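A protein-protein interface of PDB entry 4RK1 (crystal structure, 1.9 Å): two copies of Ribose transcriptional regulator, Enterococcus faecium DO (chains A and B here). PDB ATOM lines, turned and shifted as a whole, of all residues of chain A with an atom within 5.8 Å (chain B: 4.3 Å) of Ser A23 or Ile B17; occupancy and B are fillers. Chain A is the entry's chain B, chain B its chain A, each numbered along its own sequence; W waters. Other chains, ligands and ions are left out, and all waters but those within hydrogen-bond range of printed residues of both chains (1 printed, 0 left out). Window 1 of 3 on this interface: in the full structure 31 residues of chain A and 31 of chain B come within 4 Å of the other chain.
Among the printed residues, pairs that only touch across the chains: Ile A17 with Ile B17 (3.7 Å), Ile A17 with Ser B23 (3.6 Å), Ser A23 with Ile B17 (3.6 Å), Ser A23 with Thr B18 (3.9 Å), Arg A27 with Thr B18 (3.3 Å) and Glu A30 with Asn B44 (3.1 Å).
Ile A17 touches its own counterpart, Ile B17. Ile A17 touches Ser B23, and with the chains exchanged Ser A23 touches Ile B17. Leu A42 touches its own counterpart, Leu B42. Of the 7 pairs that touch across the chains among the printed residues, 4 have their exchanged pair printed and touching as well.
Water W1 lies within hydrogen-bond range of OE2 of Glu A30 (2.8 Å) and N of Asn B44 (2.9 Å).
The side-chain carboxylate (OD1) of Asp B16 sits at hydrogen-bond distance from the side-chain hydroxyl (OG1) of Thr B18. The backbone NH (N) of Asp B16 lies close to the side-chain amide oxygen (OD1) of Asn B44, at 3.3 Å. OD1 of Asn B44 lies within hydrogen-bond range of N of Ile B17 (2.6 Å). The backbone carbonyl oxygen (O) of Pro A20 sits at hydrogen-bond distance from the side-chain hydroxyl (OG) of Ser A23 (3.2 Å).
O of Leu B42 is in hydrogen-bond range of N of Leu A42 (2.8 Å).
Of the 14 printed residues of chain A, 5 touch a printed residue of chain B. Hydrophobic or aromatic side chains of chain A within 4 Å of the printed part of chain B: Ile A17 and Leu A42. Of the 8 printed residues of chain B, 5 touch a printed residue of chain A. Hydrophobic or aromatic side chains of chain B that line the printed part of chain A: Ile B17 and Leu B42.
Phe A21 touches none of the printed residues of chain B. Ser A23 touches just these residues of chain B: Ile B17 and Thr B18. Of the printed residues of chain B, Leu A42 touches Leu B42 (2.8 Å). Ile B17 touches two residues of chain A. Printed residues of chain A within 4 Å of Ser B23: Ile A17. Printed residues of chain A within 4 Å of Leu B42: Leu A42. The nearest residue of chain A that does not touch Ile B17 is Met A26 (4.4 Å).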
ATOM      1  N   ASP A  16     -21.837 -19.117  -2.074  1.00  0.00           N
ATOM      2  CA  ASP A  16     -22.151 -20.542  -2.163  1.00  0.00           C
ATOM      3  C   ASP A  16     -23.369 -20.914  -1.318  1.00  0.00           C
ATOM      4  O   ASP A  16     -23.237 -21.237  -0.137  1.00  0.00           O
ATOM      5  CB  ASP A  16     -20.927 -21.341  -1.701  1.00  0.00           C
ATOM      6  CG  ASP A  16     -21.138 -22.847  -1.751  1.00  0.00           C
ATOM      7  OD1 ASP A  16     -22.139 -23.326  -2.329  1.00  0.00           O
ATOM      8  OD2 ASP A  16     -20.275 -23.556  -1.199  1.00  0.00           O
ATOM      9  N   ILE A  17     -24.546 -20.923  -1.935  1.00  0.00           N
ATOM     10  CA  ILE A  17     -25.784 -21.311  -1.234  1.00  0.00           C
ATOM     11  C   ILE A  17     -25.825 -22.782  -0.769  1.00  0.00           C
ATOM     12  O   ILE A  17     -26.584 -23.120   0.133  1.00  0.00           O
ATOM     13  CB  ILE A  17     -27.051 -20.964  -2.063  1.00  0.00           C
ATOM     14  CG1 ILE A  17     -28.321 -21.065  -1.207  1.00  0.00           C
ATOM     15  CG2 ILE A  17     -27.169 -21.844  -3.302  1.00  0.00           C
ATOM     16  CD1 ILE A  17     -28.258 -20.303   0.104  1.00  0.00           C
ATOM     17  N   ASN A  19     -23.542 -24.250   0.906  1.00  0.00           N
ATOM     18  CA  ASN A  19     -22.869 -24.341   2.197  1.00  0.00           C
ATOM     19  C   ASN A  19     -23.846 -23.934   3.290  1.00  0.00           C
ATOM     20  O   ASN A  19     -24.398 -22.833   3.235  1.00  0.00           O
ATOM     21  CB  ASN A  19     -21.667 -23.415   2.198  1.00  0.00           C
ATOM     22  CG  ASN A  19     -20.854 -23.489   3.471  1.00  0.00           C
ATOM     23  OD1 ASN A  19     -21.291 -23.963   4.526  1.00  0.00           O
ATOM     24  ND2 ASN A  19     -19.651 -22.988   3.376  1.00  0.00           N
ATOM     25  N   PRO A  20     -24.064 -24.806   4.289  1.00  0.00           N
ATOM     26  CA  PRO A  20     -25.007 -24.455   5.370  1.00  0.00           C
ATOM     27  C   PRO A  20     -24.706 -23.133   6.096  1.00  0.00           C
ATOM     28  O   PRO A  20     -25.627 -22.505   6.638  1.00  0.00           O
ATOM     29  CB  PRO A  20     -24.889 -25.649   6.332  1.00  0.00           C
ATOM     30  CG  PRO A  20     -24.459 -26.776   5.465  1.00  0.00           C
ATOM     31  CD  PRO A  20     -23.526 -26.170   4.460  1.00  0.00           C
ATOM     32  N   PHE A  21     -23.435 -22.720   6.123  1.00  0.00           N
ATOM     33  CA  PHE A  21     -23.079 -21.418   6.653  1.00  0.00           C
ATOM     34  C   PHE A  21     -23.920 -20.312   6.009  1.00  0.00           C
ATOM     35  O   PHE A  21     -24.486 -19.480   6.707  1.00  0.00           O
ATOM     36  CB  PHE A  21     -21.573 -21.125   6.465  1.00  0.00           C
ATOM     37  CG  PHE A  21     -21.176 -19.759   6.927  1.00  0.00           C
ATOM     38  CD1 PHE A  21     -20.875 -19.529   8.262  1.00  0.00           C
ATOM     39  CD2 PHE A  21     -21.178 -18.681   6.052  1.00  0.00           C
ATOM     40  CE1 PHE A  21     -20.559 -18.259   8.707  1.00  0.00           C
ATOM     41  CE2 PHE A  21     -20.865 -17.406   6.497  1.00  0.00           C
ATOM     42  CZ  PHE A  21     -20.544 -17.200   7.830  1.00  0.00           C
ATOM     43  N   PHE A  22     -24.008 -20.305   4.679  1.00  0.00           N
ATOM     44  CA  PHE A  22     -24.692 -19.221   3.978  1.00  0.00           C
ATOM     45  C   PHE A  22     -26.202 -19.346   4.019  1.00  0.00           C
ATOM     46  O   PHE A  22     -26.892 -18.331   4.014  1.00  0.00           O
ATOM     47  CB  PHE A  22     -24.178 -19.081   2.552  1.00  0.00           C
ATOM     48  CG  PHE A  22     -22.769 -18.607   2.499  1.00  0.00           C
ATOM     49  CD1 PHE A  22     -22.459 -17.325   2.914  1.00  0.00           C
ATOM     50  CD2 PHE A  22     -21.749 -19.453   2.106  1.00  0.00           C
ATOM     51  CE1 PHE A  22     -21.155 -16.884   2.920  1.00  0.00           C
ATOM     52  CE2 PHE A  22     -20.440 -19.014   2.099  1.00  0.00           C
ATOM     53  CZ  PHE A  22     -20.144 -17.736   2.515  1.00  0.00           C
ATOM     54  N   SER A  23     -26.724 -20.569   4.098  1.00  0.00           N
ATOM     55  CA  SER A  23     -28.173 -20.721   4.247  1.00  0.00           C
ATOM     56  C   SER A  23     -28.603 -20.341   5.673  1.00  0.00           C
ATOM     57  O   SER A  23     -29.643 -19.720   5.856  1.00  0.00           O
ATOM     58  CB  SER A  23     -28.659 -22.113   3.826  1.00  0.00           C
ATOM     59  OG  SER A  23     -27.950 -23.139   4.473  1.00  0.00           O
ATOM     60  N   THR A  24     -27.790 -20.656   6.675  1.00  0.00           N
ATOM     61  CA  THR A  24     -28.092 -20.210   8.035  1.00  0.00           C
ATOM     62  C   THR A  24     -27.950 -18.693   8.169  1.00  0.00           C
ATOM     63  O   THR A  24     -28.728 -18.068   8.879  1.00  0.00           O
ATOM     64  CB  THR A  24     -27.229 -20.944   9.069  1.00  0.00           C
ATOM     65  OG1 THR A  24     -27.569 -22.332   9.045  1.00  0.00           O
ATOM     66  CG2 THR A  24     -27.465 -20.404  10.463  1.00  0.00           C
ATOM     67  N   LEU A  25     -26.958 -18.111   7.489  1.00  0.00           N
ATOM     68  CA  LEU A  25     -26.803 -16.661   7.438  1.00  0.00           C
ATOM     69  C   LEU A  25     -28.074 -16.022   6.912  1.00  0.00           C
ATOM     70  O   LEU A  25     -28.606 -15.081   7.499  1.00  0.00           O
ATOM     71  CB  LEU A  25     -25.641 -16.278   6.531  1.00  0.00           C
ATOM     72  CG  LEU A  25     -25.387 -14.774   6.381  1.00  0.00           C
ATOM     73  CD1 LEU A  25     -24.615 -14.272   7.594  1.00  0.00           C
ATOM     74  CD2 LEU A  25     -24.612 -14.504   5.105  1.00  0.00           C
ATOM     75  N   MET A  26     -28.554 -16.555   5.798  1.00  0.00           N
ATOM     76  CA  MET A  26     -29.805 -16.102   5.201  1.00  0.00           C
ATOM     77  C   MET A  26     -30.970 -16.169   6.132  1.00  0.00           C
ATOM     78  O   MET A  26     -31.764 -15.234   6.194  1.00  0.00           O
ATOM     79  CB  MET A  26     -30.129 -16.947   3.982  1.00  0.00           C
ATOM     80  CG  MET A  26     -29.956 -16.092   2.761  1.00  0.00           C
ATOM     81  SD  MET A  26     -31.583 -15.011   2.637  1.00  0.00           S
ATOM     82  CE  MET A  26     -32.494 -16.528   1.724  1.00  0.00           C
ATOM     83  N   ARG A  27     -31.098 -17.268   6.862  1.00  0.00           N
ATOM     84  CA  ARG A  27     -32.171 -17.391   7.863  1.00  0.00           C
ATOM     85  C   ARG A  27     -32.100 -16.293   8.925  1.00  0.00           C
ATOM     86  O   ARG A  27     -33.130 -15.782   9.356  1.00  0.00           O
ATOM     87  CB  ARG A  27     -32.149 -18.770   8.543  1.00  0.00           C
ATOM     88  CG  ARG A  27     -33.065 -19.798   7.891  1.00  0.00           C
ATOM     89  CD  ARG A  27     -33.203 -21.063   8.734  1.00  0.00           C
ATOM     90  NE  ARG A  27     -33.735 -20.817  10.080  1.00  0.00           N
ATOM     91  CZ  ARG A  27     -33.039 -20.885  11.219  1.00  0.00           C
ATOM     92  NH1 ARG A  27     -33.649 -20.633  12.372  1.00  0.00           N
ATOM     93  NH2 ARG A  27     -31.744 -21.203  11.229  1.00  0.00           N
ATOM     94  N   GLY A  28     -30.891 -15.932   9.358  1.00  0.00           N
ATOM     95  CA  GLY A  28     -30.735 -14.852  10.333  1.00  0.00           C
ATOM     96  C   GLY A  28     -31.158 -13.504   9.765  1.00  0.00           C
ATOM     97  O   GLY A  28     -31.808 -12.710  10.437  1.00  0.00           O
ATOM     98  N   GLU A  30     -33.329 -13.072   7.194  1.00  0.00           N
ATOM     99  CA  GLU A  30     -34.787 -13.162   7.018  1.00  0.00           C
ATOM    100  C   GLU A  30     -35.534 -12.939   8.321  1.00  0.00           C
ATOM    101  O   GLU A  30     -36.593 -12.309   8.339  1.00  0.00           O
ATOM    102  CB  GLU A  30     -35.183 -14.532   6.466  1.00  0.00           C
ATOM    103  CG  GLU A  30     -34.808 -14.750   5.018  1.00  0.00           C
ATOM    104  CD  GLU A  30     -35.021 -16.184   4.583  1.00  0.00           C
ATOM    105  OE1 GLU A  30     -35.199 -17.059   5.459  1.00  0.00           O
ATOM    106  OE2 GLU A  30     -35.008 -16.433   3.364  1.00  0.00           O
ATOM    107  N   LEU A  42     -32.184 -14.138  -2.435  1.00  0.00           N
ATOM    108  CA  LEU A  42     -30.792 -14.571  -2.419  1.00  0.00           C
ATOM    109  C   LEU A  42     -30.273 -14.884  -3.814  1.00  0.00           C
ATOM    110  O   LEU A  42     -30.958 -15.498  -4.636  1.00  0.00           O
ATOM    111  CB  LEU A  42     -30.624 -15.791  -1.524  1.00  0.00           C
ATOM    112  CG  LEU A  42     -29.190 -16.333  -1.537  1.00  0.00           C
ATOM    113  CD1 LEU A  42     -28.687 -16.565  -0.132  1.00  0.00           C
ATOM    114  CD2 LEU A  42     -29.067 -17.593  -2.384  1.00  0.00           C
ATOM    115  N   VAL B  14     -38.740 -21.602  -2.722  1.00  0.00           N
ATOM    116  CA  VAL B  14     -38.602 -22.903  -2.076  1.00  0.00           C
ATOM    117  C   VAL B  14     -39.127 -22.864  -0.636  1.00  0.00           C
ATOM    118  O   VAL B  14     -39.189 -21.808  -0.025  1.00  0.00           O
ATOM    119  CB  VAL B  14     -37.153 -23.417  -2.096  1.00  0.00           C
ATOM    120  CG1 VAL B  14     -36.655 -23.549  -3.528  1.00  0.00           C
ATOM    121  CG2 VAL B  14     -36.228 -22.541  -1.265  1.00  0.00           C
ATOM    122  N   ASP B  16     -37.695 -24.275   1.991  1.00  0.00           N
ATOM    123  CA  ASP B  16     -36.640 -24.412   3.001  1.00  0.00           C
ATOM    124  C   ASP B  16     -35.229 -24.401   2.404  1.00  0.00           C
ATOM    125  O   ASP B  16     -34.669 -25.452   2.083  1.00  0.00           O
ATOM    126  CB  ASP B  16     -36.859 -25.722   3.788  1.00  0.00           C
ATOM    127  CG  ASP B  16     -35.802 -25.954   4.870  1.00  0.00           C
ATOM    128  OD1 ASP B  16     -35.027 -25.020   5.181  1.00  0.00           O
ATOM    129  OD2 ASP B  16     -35.738 -27.084   5.403  1.00  0.00           O
ATOM    130  N   ILE B  17     -34.627 -23.222   2.327  1.00  0.00           N
ATOM    131  CA  ILE B  17     -33.275 -23.084   1.766  1.00  0.00           C
ATOM    132  C   ILE B  17     -32.164 -23.777   2.579  1.00  0.00           C
ATOM    133  O   ILE B  17     -31.096 -24.080   2.031  1.00  0.00           O
ATOM    134  CB  ILE B  17     -32.921 -21.598   1.492  1.00  0.00           C
ATOM    135  CG1 ILE B  17     -31.678 -21.485   0.597  1.00  0.00           C
ATOM    136  CG2 ILE B  17     -32.732 -20.814   2.786  1.00  0.00           C
ATOM    137  CD1 ILE B  17     -31.726 -22.341  -0.656  1.00  0.00           C
ATOM    138  N   THR B  18     -32.427 -24.085   3.851  1.00  0.00           N
ATOM    139  CA  THR B  18     -31.442 -24.780   4.694  1.00  0.00           C
ATOM    140  C   THR B  18     -31.346 -26.265   4.380  1.00  0.00           C
ATOM    141  O   THR B  18     -30.430 -26.923   4.834  1.00  0.00           O
ATOM    142  CB  THR B  18     -31.726 -24.614   6.207  1.00  0.00           C
ATOM    143  OG1 THR B  18     -32.852 -25.403   6.596  1.00  0.00           O
ATOM    144  CG2 THR B  18     -31.972 -23.163   6.553  1.00  0.00           C
ATOM    145  N   ASN B  19     -32.290 -26.794   3.612  1.00  0.00           N
ATOM    146  CA  ASN B  19     -32.243 -28.192   3.182  1.00  0.00           C
ATOM    147  C   ASN B  19     -31.399 -28.323   1.913  1.00  0.00           C
ATOM    148  O   ASN B  19     -31.720 -27.707   0.900  1.00  0.00           O
ATOM    149  CB  ASN B  19     -33.659 -28.669   2.905  1.00  0.00           C
ATOM    150  CG  ASN B  19     -33.752 -30.155   2.614  1.00  0.00           C
ATOM    151  OD1 ASN B  19     -32.785 -30.840   2.299  1.00  0.00           O
ATOM    152  ND2 ASN B  19     -34.952 -30.654   2.715  1.00  0.00           N
ATOM    153  N   SER B  23     -31.075 -26.276  -2.085  1.00  0.00           N
ATOM    154  CA  SER B  23     -29.901 -25.584  -2.609  1.00  0.00           C
ATOM    155  C   SER B  23     -29.326 -26.298  -3.849  1.00  0.00           C
ATOM    156  O   SER B  23     -28.867 -25.644  -4.784  1.00  0.00           O
ATOM    157  CB  SER B  23     -28.838 -25.364  -1.516  1.00  0.00           C
ATOM    158  OG  SER B  23     -28.471 -26.550  -0.848  1.00  0.00           O
ATOM    159  N   LEU B  42     -33.457 -16.492  -5.327  1.00  0.00           N
ATOM    160  CA  LEU B  42     -34.145 -17.463  -4.506  1.00  0.00           C
ATOM    161  C   LEU B  42     -34.831 -16.819  -3.306  1.00  0.00           C
ATOM    162  O   LEU B  42     -34.263 -15.957  -2.646  1.00  0.00           O
ATOM    163  CB  LEU B  42     -33.180 -18.556  -4.060  1.00  0.00           C
ATOM    164  CG  LEU B  42     -33.899 -19.544  -3.130  1.00  0.00           C
ATOM    165  CD1 LEU B  42     -33.844 -20.970  -3.635  1.00  0.00           C
ATOM    166  CD2 LEU B  42     -33.393 -19.421  -1.700  1.00  0.00           C
ATOM    167  N   ASN B  44     -37.030 -17.995   0.235  1.00  0.00           N
ATOM    168  CA  ASN B  44     -37.439 -19.004   1.190  1.00  0.00           C
ATOM    169  C   ASN B  44     -38.835 -18.604   1.636  1.00  0.00           C
ATOM    170  O   ASN B  44     -38.996 -17.602   2.328  1.00  0.00           O
ATOM    171  CB  ASN B  44     -36.468 -18.979   2.380  1.00  0.00           C
ATOM    172  CG  ASN B  44     -36.529 -20.230   3.225  1.00  0.00           C
ATOM    173  OD1 ASN B  44     -36.337 -21.330   2.722  1.00  0.00           O
ATOM    174  ND2 ASN B  44     -36.756 -20.066   4.523  1.00  0.00           N
HETATM  175  O   HOH W   1     -36.663 -15.394   1.387  1.00  0.00           O
